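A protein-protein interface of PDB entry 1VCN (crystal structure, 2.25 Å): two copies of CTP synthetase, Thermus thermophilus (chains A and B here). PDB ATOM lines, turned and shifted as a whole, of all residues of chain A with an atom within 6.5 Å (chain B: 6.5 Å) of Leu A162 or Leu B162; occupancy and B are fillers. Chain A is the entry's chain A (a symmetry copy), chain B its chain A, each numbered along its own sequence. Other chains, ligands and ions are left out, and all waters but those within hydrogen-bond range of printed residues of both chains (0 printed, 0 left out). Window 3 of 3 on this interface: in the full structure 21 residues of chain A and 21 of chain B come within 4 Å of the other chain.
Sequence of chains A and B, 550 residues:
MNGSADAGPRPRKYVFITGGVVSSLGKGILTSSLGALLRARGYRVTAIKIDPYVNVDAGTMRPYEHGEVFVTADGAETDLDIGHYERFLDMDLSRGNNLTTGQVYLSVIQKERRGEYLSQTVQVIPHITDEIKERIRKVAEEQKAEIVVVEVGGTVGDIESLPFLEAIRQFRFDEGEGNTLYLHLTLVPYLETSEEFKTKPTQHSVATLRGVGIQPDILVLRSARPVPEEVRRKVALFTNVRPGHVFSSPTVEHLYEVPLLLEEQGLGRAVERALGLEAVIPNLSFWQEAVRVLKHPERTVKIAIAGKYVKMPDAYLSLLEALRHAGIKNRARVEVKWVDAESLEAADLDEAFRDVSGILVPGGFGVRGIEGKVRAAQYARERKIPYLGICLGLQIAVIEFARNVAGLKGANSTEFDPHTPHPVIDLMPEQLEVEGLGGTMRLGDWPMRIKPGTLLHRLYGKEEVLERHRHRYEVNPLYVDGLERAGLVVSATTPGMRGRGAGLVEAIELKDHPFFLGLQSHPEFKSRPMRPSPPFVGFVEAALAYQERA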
ATOM      1  N   VAL A 124     -10.095 -33.147  20.638  1.00  0.00           N
ATOM      2  CA  VAL A 124     -11.323 -33.463  21.361  1.00  0.00           C
ATOM      3  C   VAL A 124     -11.556 -34.964  21.237  1.00  0.00           C
ATOM      4  O   VAL A 124     -11.834 -35.650  22.222  1.00  0.00           O
ATOM      5  CB  VAL A 124     -12.515 -32.661  20.777  1.00  0.00           C
ATOM      6  CG1 VAL A 124     -13.825 -33.092  21.411  1.00  0.00           C
ATOM      7  CG2 VAL A 124     -12.285 -31.180  21.038  1.00  0.00           C
ATOM      8  N   THR A 129     -12.557 -37.317  24.678  1.00  0.00           N
ATOM      9  CA  THR A 129     -13.520 -38.401  24.802  1.00  0.00           C
ATOM     10  C   THR A 129     -12.944 -39.565  25.602  1.00  0.00           C
ATOM     11  O   THR A 129     -13.651 -40.152  26.423  1.00  0.00           O
ATOM     12  CB  THR A 129     -14.044 -38.880  23.415  1.00  0.00           C
ATOM     13  OG1 THR A 129     -12.968 -38.948  22.479  1.00  0.00           O
ATOM     14  CG2 THR A 129     -15.096 -37.896  22.879  1.00  0.00           C
ATOM     15  N   GLY A 157     -28.142 -31.528  21.154  1.00  0.00           N
ATOM     16  CA  GLY A 157     -28.121 -30.501  20.128  1.00  0.00           C
ATOM     17  C   GLY A 157     -27.128 -29.390  20.438  1.00  0.00           C
ATOM     18  O   GLY A 157     -26.338 -28.994  19.581  1.00  0.00           O
ATOM     19  N   ASP A 158     -27.166 -28.887  21.668  1.00  0.00           N
ATOM     20  CA  ASP A 158     -26.257 -27.822  22.085  1.00  0.00           C
ATOM     21  C   ASP A 158     -24.835 -28.348  21.931  1.00  0.00           C
ATOM     22  O   ASP A 158     -24.594 -29.538  22.130  1.00  0.00           O
ATOM     23  CB  ASP A 158     -26.567 -27.439  23.527  1.00  0.00           C
ATOM     24  CG  ASP A 158     -27.989 -26.915  23.688  1.00  0.00           C
ATOM     25  OD1 ASP A 158     -28.473 -26.828  24.835  1.00  0.00           O
ATOM     26  OD2 ASP A 158     -28.624 -26.587  22.655  1.00  0.00           O
ATOM     27  N   ILE A 159     -23.888 -27.480  21.581  1.00  0.00           N
ATOM     28  CA  ILE A 159     -22.539 -27.962  21.352  1.00  0.00           C
ATOM     29  C   ILE A 159     -21.750 -28.363  22.579  1.00  0.00           C
ATOM     30  O   ILE A 159     -20.799 -29.130  22.475  1.00  0.00           O
ATOM     31  CB  ILE A 159     -21.710 -26.972  20.486  1.00  0.00           C
ATOM     32  CG1 ILE A 159     -21.242 -25.769  21.295  1.00  0.00           C
ATOM     33  CG2 ILE A 159     -22.560 -26.484  19.315  1.00  0.00           C
ATOM     34  CD1 ILE A 159     -20.388 -24.802  20.459  1.00  0.00           C
ATOM     35  N   GLU A 160     -22.152 -27.880  23.746  1.00  0.00           N
ATOM     36  CA  GLU A 160     -21.438 -28.242  24.964  1.00  0.00           C
ATOM     37  C   GLU A 160     -21.531 -29.737  25.289  1.00  0.00           C
ATOM     38  O   GLU A 160     -20.661 -30.278  25.948  1.00  0.00           O
ATOM     39  CB  GLU A 160     -21.951 -27.414  26.145  1.00  0.00           C
ATOM     40  CG  GLU A 160     -23.458 -27.234  26.164  1.00  0.00           C
ATOM     41  CD  GLU A 160     -23.901 -26.264  27.235  1.00  0.00           C
ATOM     42  OE1 GLU A 160     -23.219 -25.225  27.397  1.00  0.00           O
ATOM     43  OE2 GLU A 160     -24.927 -26.529  27.904  1.00  0.00           O
ATOM     44  N   SER A 161     -22.570 -30.408  24.809  1.00  0.00           N
ATOM     45  CA  SER A 161     -22.732 -31.829  25.097  1.00  0.00           C
ATOM     46  C   SER A 161     -22.088 -32.766  24.087  1.00  0.00           C
ATOM     47  O   SER A 161     -21.948 -33.959  24.358  1.00  0.00           O
ATOM     48  CB  SER A 161     -24.219 -32.174  25.216  1.00  0.00           C
ATOM     49  OG  SER A 161     -24.904 -31.901  24.010  1.00  0.00           O
ATOM     50  N   LEU A 162     -21.672 -32.232  22.943  1.00  0.00           N
ATOM     51  CA  LEU A 162     -21.085 -33.057  21.895  1.00  0.00           C
ATOM     52  C   LEU A 162     -19.963 -34.007  22.331  1.00  0.00           C
ATOM     53  O   LEU A 162     -19.986 -35.174  21.979  1.00  0.00           O
ATOM     54  CB  LEU A 162     -20.617 -32.178  20.717  1.00  0.00           C
ATOM     55  CG  LEU A 162     -21.582 -31.887  19.544  1.00  0.00           C
ATOM     56  CD1 LEU A 162     -23.016 -32.142  19.934  1.00  0.00           C
ATOM     57  CD2 LEU A 162     -21.405 -30.437  19.073  1.00  0.00           C
ATOM     58  N   PRO A 163     -18.970 -33.520  23.092  1.00  0.00           N
ATOM     59  CA  PRO A 163     -17.893 -34.431  23.510  1.00  0.00           C
ATOM     60  C   PRO A 163     -18.425 -35.570  24.378  1.00  0.00           C
ATOM     61  O   PRO A 163     -17.923 -36.693  24.322  1.00  0.00           O
ATOM     62  CB  PRO A 163     -16.941 -33.516  24.281  1.00  0.00           C
ATOM     63  CG  PRO A 163     -17.177 -32.168  23.647  1.00  0.00           C
ATOM     64  CD  PRO A 163     -18.683 -32.146  23.518  1.00  0.00           C
ATOM     65  N   PHE A 164     -19.456 -35.276  25.166  1.00  0.00           N
ATOM     66  CA  PHE A 164     -20.039 -36.288  26.035  1.00  0.00           C
ATOM     67  C   PHE A 164     -20.907 -37.278  25.267  1.00  0.00           C
ATOM     68  O   PHE A 164     -20.935 -38.474  25.589  1.00  0.00           O
ATOM     69  CB  PHE A 164     -20.839 -35.613  27.153  1.00  0.00           C
ATOM     70  CG  PHE A 164     -19.976 -34.864  28.132  1.00  0.00           C
ATOM     71  CD1 PHE A 164     -19.154 -35.557  29.022  1.00  0.00           C
ATOM     72  CD2 PHE A 164     -19.940 -33.469  28.128  1.00  0.00           C
ATOM     73  CE1 PHE A 164     -18.307 -34.876  29.888  1.00  0.00           C
ATOM     74  CE2 PHE A 164     -19.096 -32.779  28.992  1.00  0.00           C
ATOM     75  CZ  PHE A 164     -18.274 -33.488  29.874  1.00  0.00           C
ATOM     76  N   LEU A 165     -21.610 -36.788  24.250  1.00  0.00           N
ATOM     77  CA  LEU A 165     -22.453 -37.661  23.443  1.00  0.00           C
ATOM     78  C   LEU A 165     -21.578 -38.633  22.647  1.00  0.00           C
ATOM     79  O   LEU A 165     -21.908 -39.810  22.530  1.00  0.00           O
ATOM     80  CB  LEU A 165     -23.335 -36.828  22.515  1.00  0.00           C
ATOM     81  CG  LEU A 165     -24.356 -35.973  23.265  1.00  0.00           C
ATOM     82  CD1 LEU A 165     -25.175 -35.138  22.272  1.00  0.00           C
ATOM     83  CD2 LEU A 165     -25.283 -36.894  24.084  1.00  0.00           C
ATOM     84  N   GLU A 166     -20.454 -38.141  22.123  1.00  0.00           N
ATOM     85  CA  GLU A 166     -19.526 -38.992  21.367  1.00  0.00           C
ATOM     86  C   GLU A 166     -18.883 -40.033  22.294  1.00  0.00           C
ATOM     87  O   GLU A 166     -18.647 -41.177  21.897  1.00  0.00           O
ATOM     88  CB  GLU A 166     -18.443 -38.137  20.692  1.00  0.00           C
ATOM     89  CG  GLU A 166     -17.260 -38.914  20.061  1.00  0.00           C
ATOM     90  CD  GLU A 166     -17.693 -39.983  19.060  1.00  0.00           C
ATOM     91  OE1 GLU A 166     -18.755 -39.827  18.429  1.00  0.00           O
ATOM     92  OE2 GLU A 166     -16.970 -40.992  18.898  1.00  0.00           O
ATOM     93  N   ALA A 167     -18.614 -39.631  23.534  1.00  0.00           N
ATOM     94  CA  ALA A 167     -18.014 -40.535  24.496  1.00  0.00           C
ATOM     95  C   ALA A 167     -18.969 -41.678  24.848  1.00  0.00           C
ATOM     96  O   ALA A 167     -18.580 -42.844  24.839  1.00  0.00           O
ATOM     97  CB  ALA A 167     -17.619 -39.778  25.756  1.00  0.00           C
ATOM     98  N   VAL A 212     -25.532 -37.507  15.740  1.00  0.00           N
ATOM     99  CA  VAL A 212     -24.259 -37.611  16.438  1.00  0.00           C
ATOM    100  C   VAL A 212     -23.929 -39.085  16.591  1.00  0.00           C
ATOM    101  O   VAL A 212     -23.021 -39.460  17.325  1.00  0.00           O
ATOM    102  CB  VAL A 212     -24.278 -36.881  17.827  1.00  0.00           C
ATOM    103  CG1 VAL A 212     -24.611 -35.412  17.622  1.00  0.00           C
ATOM    104  CG2 VAL A 212     -25.276 -37.524  18.770  1.00  0.00           C
ATOM    105  N   VAL B 124     -20.016 -22.873  26.981  1.00  0.00           N
ATOM    106  CA  VAL B 124     -19.228 -22.679  25.768  1.00  0.00           C
ATOM    107  C   VAL B 124     -19.675 -21.368  25.134  1.00  0.00           C
ATOM    108  O   VAL B 124     -18.855 -20.530  24.754  1.00  0.00           O
ATOM    109  CB  VAL B 124     -19.434 -23.869  24.795  1.00  0.00           C
ATOM    110  CG1 VAL B 124     -18.747 -23.612  23.466  1.00  0.00           C
ATOM    111  CG2 VAL B 124     -18.859 -25.127  25.430  1.00  0.00           C
ATOM    112  N   THR B 129     -16.794 -18.492  23.787  1.00  0.00           N
ATOM    113  CA  THR B 129     -16.803 -17.678  22.582  1.00  0.00           C
ATOM    114  C   THR B 129     -16.391 -16.240  22.880  1.00  0.00           C
ATOM    115  O   THR B 129     -15.646 -15.642  22.102  1.00  0.00           O
ATOM    116  CB  THR B 129     -18.179 -17.727  21.852  1.00  0.00           C
ATOM    117  OG1 THR B 129     -19.242 -17.655  22.801  1.00  0.00           O
ATOM    118  CG2 THR B 129     -18.313 -19.040  21.065  1.00  0.00           C
ATOM    119  N   GLY B 157     -16.654 -28.571  10.105  1.00  0.00           N
ATOM    120  CA  GLY B 157     -17.398 -29.799  10.327  1.00  0.00           C
ATOM    121  C   GLY B 157     -16.969 -30.516  11.599  1.00  0.00           C
ATOM    122  O   GLY B 157     -17.807 -30.925  12.404  1.00  0.00           O
ATOM    123  N   ASP B 158     -15.662 -30.665  11.785  1.00  0.00           N
ATOM    124  CA  ASP B 158     -15.130 -31.331  12.972  1.00  0.00           C
ATOM    125  C   ASP B 158     -15.599 -30.540  14.188  1.00  0.00           C
ATOM    126  O   ASP B 158     -15.726 -29.318  14.116  1.00  0.00           O
ATOM    127  CB  ASP B 158     -13.610 -31.378  12.878  1.00  0.00           C
ATOM    128  CG  ASP B 158     -13.135 -32.164  11.663  1.00  0.00           C
ATOM    129  OD1 ASP B 158     -11.945 -32.055  11.302  1.00  0.00           O
ATOM    130  OD2 ASP B 158     -13.962 -32.899  11.067  1.00  0.00           O
ATOM    131  N   ILE B 159     -15.858 -31.217  15.304  1.00  0.00           N
ATOM    132  CA  ILE B 159     -16.379 -30.504  16.456  1.00  0.00           C
ATOM    133  C   ILE B 159     -15.404 -29.613  17.194  1.00  0.00           C
ATOM    134  O   ILE B 159     -15.818 -28.697  17.896  1.00  0.00           O
ATOM    135  CB  ILE B 159     -17.088 -31.461  17.456  1.00  0.00           C
ATOM    136  CG1 ILE B 159     -16.086 -32.256  18.284  1.00  0.00           C
ATOM    137  CG2 ILE B 159     -17.980 -32.433  16.687  1.00  0.00           C
ATOM    138  CD1 ILE B 159     -16.775 -33.177  19.304  1.00  0.00           C
ATOM    139  N   GLU B 160     -14.112 -29.849  17.019  1.00  0.00           N
ATOM    140  CA  GLU B 160     -13.126 -29.015  17.695  1.00  0.00           C
ATOM    141  C   GLU B 160     -13.159 -27.555  17.229  1.00  0.00           C
ATOM    142  O   GLU B 160     -12.774 -26.666  17.967  1.00  0.00           O
ATOM    143  CB  GLU B 160     -11.721 -29.595  17.507  1.00  0.00           C
ATOM    144  CG  GLU B 160     -11.454 -30.120  16.107  1.00  0.00           C
ATOM    145  CD  GLU B 160     -10.131 -30.845  16.016  1.00  0.00           C
ATOM    146  OE1 GLU B 160      -9.820 -31.609  16.961  1.00  0.00           O
ATOM    147  OE2 GLU B 160      -9.411 -30.665  15.006  1.00  0.00           O
ATOM    148  N   SER B 161     -13.639 -27.306  16.018  1.00  0.00           N
ATOM    149  CA  SER B 161     -13.680 -25.941  15.502  1.00  0.00           C
ATOM    150  C   SER B 161     -14.964 -25.182  15.800  1.00  0.00           C
ATOM    151  O   SER B 161     -15.008 -23.963  15.636  1.00  0.00           O
ATOM    152  CB  SER B 161     -13.444 -25.944  13.990  1.00  0.00           C
ATOM    153  OG  SER B 161     -14.444 -26.685  13.319  1.00  0.00           O
ATOM    154  N   LEU B 162     -15.992 -25.886  16.262  1.00  0.00           N
ATOM    155  CA  LEU B 162     -17.277 -25.255  16.531  1.00  0.00           C
ATOM    156  C   LEU B 162     -17.240 -23.984  17.388  1.00  0.00           C
ATOM    157  O   LEU B 162     -17.855 -22.993  17.028  1.00  0.00           O
ATOM    158  CB  LEU B 162     -18.264 -26.278  17.133  1.00  0.00           C
ATOM    159  CG  LEU B 162     -19.188 -27.095  16.200  1.00  0.00           C
ATOM    160  CD1 LEU B 162     -18.678 -27.096  14.781  1.00  0.00           C
ATOM    161  CD2 LEU B 162     -19.318 -28.531  16.724  1.00  0.00           C
ATOM    162  N   PRO B 163     -16.528 -23.996  18.526  1.00  0.00           N
ATOM    163  CA  PRO B 163     -16.492 -22.777  19.347  1.00  0.00           C
ATOM    164  C   PRO B 163     -15.859 -21.609  18.593  1.00  0.00           C
ATOM    165  O   PRO B 163     -16.251 -20.456  18.772  1.00  0.00           O
ATOM    166  CB  PRO B 163     -15.663 -23.196  20.561  1.00  0.00           C
ATOM    167  CG  PRO B 163     -15.917 -24.681  20.649  1.00  0.00           C
ATOM    168  CD  PRO B 163     -15.829 -25.096  19.199  1.00  0.00           C
ATOM    169  N   PHE B 164     -14.889 -21.920  17.736  1.00  0.00           N
ATOM    170  CA  PHE B 164     -14.216 -20.883  16.967  1.00  0.00           C
ATOM    171  C   PHE B 164     -15.073 -20.373  15.814  1.00  0.00           C
ATOM    172  O   PHE B 164     -15.046 -19.177  15.491  1.00  0.00           O
ATOM    173  CB  PHE B 164     -12.870 -21.407  16.458  1.00  0.00           C
ATOM    174  CG  PHE B 164     -11.869 -21.638  17.556  1.00  0.00           C
ATOM    175  CD1 PHE B 164     -11.292 -20.556  18.224  1.00  0.00           C
ATOM    176  CD2 PHE B 164     -11.543 -22.932  17.963  1.00  0.00           C
ATOM    177  CE1 PHE B 164     -10.413 -20.757  19.281  1.00  0.00           C
ATOM    178  CE2 PHE B 164     -10.663 -23.143  19.019  1.00  0.00           C
ATOM    179  CZ  PHE B 164     -10.098 -22.048  19.682  1.00  0.00           C
ATOM    180  N   LEU B 165     -15.836 -21.270  15.197  1.00  0.00           N
ATOM    181  CA  LEU B 165     -16.705 -20.873  14.097  1.00  0.00           C
ATOM    182  C   LEU B 165     -17.824 -19.968  14.622  1.00  0.00           C
ATOM    183  O   LEU B 165     -18.173 -18.979  13.983  1.00  0.00           O
ATOM    184  CB  LEU B 165     -17.277 -22.109  13.406  1.00  0.00           C
ATOM    185  CG  LEU B 165     -16.211 -22.952  12.706  1.00  0.00           C
ATOM    186  CD1 LEU B 165     -16.852 -24.192  12.072  1.00  0.00           C
ATOM    187  CD2 LEU B 165     -15.517 -22.095  11.628  1.00  0.00           C
ATOM    188  N   GLU B 166     -18.364 -20.297  15.797  1.00  0.00           N
ATOM    189  CA  GLU B 166     -19.421 -19.483  16.408  1.00  0.00           C
ATOM    190  C   GLU B 166     -18.868 -18.110  16.814  1.00  0.00           C
ATOM    191  O   GLU B 166     -19.556 -17.091  16.708  1.00  0.00           O
ATOM    192  CB  GLU B 166     -20.013 -20.202  17.630  1.00  0.00           C
ATOM    193  CG  GLU B 166     -20.969 -19.362  18.515  1.00  0.00           C
ATOM    194  CD  GLU B 166     -22.127 -18.735  17.742  1.00  0.00           C
ATOM    195  OE1 GLU B 166     -22.550 -19.303  16.719  1.00  0.00           O
ATOM    196  OE2 GLU B 166     -22.625 -17.663  18.156  1.00  0.00           O
ATOM    197  N   ALA B 167     -17.617 -18.089  17.268  1.00  0.00           N
ATOM    198  CA  ALA B 167     -16.992 -16.844  17.671  1.00  0.00           C
ATOM    199  C   ALA B 167     -16.796 -15.913  16.473  1.00  0.00           C
ATOM    200  O   ALA B 167     -17.138 -14.733  16.535  1.00  0.00           O
ATOM    201  CB  ALA B 167     -15.653 -17.120  18.341  1.00  0.00           C
ATOM    202  N   VAL B 212     -23.649 -23.810  10.634  1.00  0.00           N
ATOM    203  CA  VAL B 212     -23.178 -23.222  11.880  1.00  0.00           C
ATOM    204  C   VAL B 212     -23.429 -21.726  11.814  1.00  0.00           C
ATOM    205  O   VAL B 212     -22.938 -20.963  12.639  1.00  0.00           O
ATOM    206  CB  VAL B 212     -21.666 -23.537  12.155  1.00  0.00           C
ATOM    207  CG1 VAL B 212     -21.465 -25.042  12.212  1.00  0.00           C
ATOM    208  CG2 VAL B 212     -20.777 -22.925  11.091  1.00  0.00           C
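N of Thr B129 sits at hydrogen-bond distance from O of Val B124.
O of Val A124 lies within hydrogen-bond range of N of Thr A129, at 3.1 Å.
Val A124 touches Ile B159.
CB of Glu B160 touches CG2 of Val A124, at 3.9 Å.
Ile A159 touches Val B124.
Glu A160 touches Val B124.
Leu A162 touches Leu B162.
Of the printed residues of chain B, Val A124 touches Ile B159 and Glu B160.
Of the printed residues of chain B, Ile A159 touches Val B124.
Leu A162 touches just one residue of chain B: Leu B162.
Printed residues of chain A within 4 Å of Val B124: Ile A159 (3.6 Å) and Glu A160 (3.9 Å).
Printed residues of chain A within 4 Å of Ile B159: Val A124 (3.6 Å).
Of the printed residues of chain A, Glu B160 touches Val A124.
Of chain A, only Leu A162 comes within 4 Å of Leu B162.
Pro B163 touches none of the printed residues of chain A.
Ala B167 touches none of the printed residues of chain A.
The nearest printed residue of chain B that does not touch Val A124 is Ser B161 (6.5 Å).
Printed residues of chain B that touch a printed residue of chain A: Val B124, Ile B159, Glu B160 and Leu B162.
Among the printed residues, 5 pairs touch across the chains.
Among the printed residues, no Asp or Glu carboxylate lies within 4 Å of a Lys or Arg side-chain nitrogen of the other chain.
Val A124 touches Ile B159, and with the chains exchanged Ile A159 touches Val B124.
Val A124 touches Glu B160, and with the chains exchanged Glu A160 touches Val B124.
Leu B162 touches its own counterpart, Leu A162.
14 positions are printed for both chains.
Of the 5 pairs that touch across the chains among the printed residues, 5 have their exchanged pair printed and touching as well.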
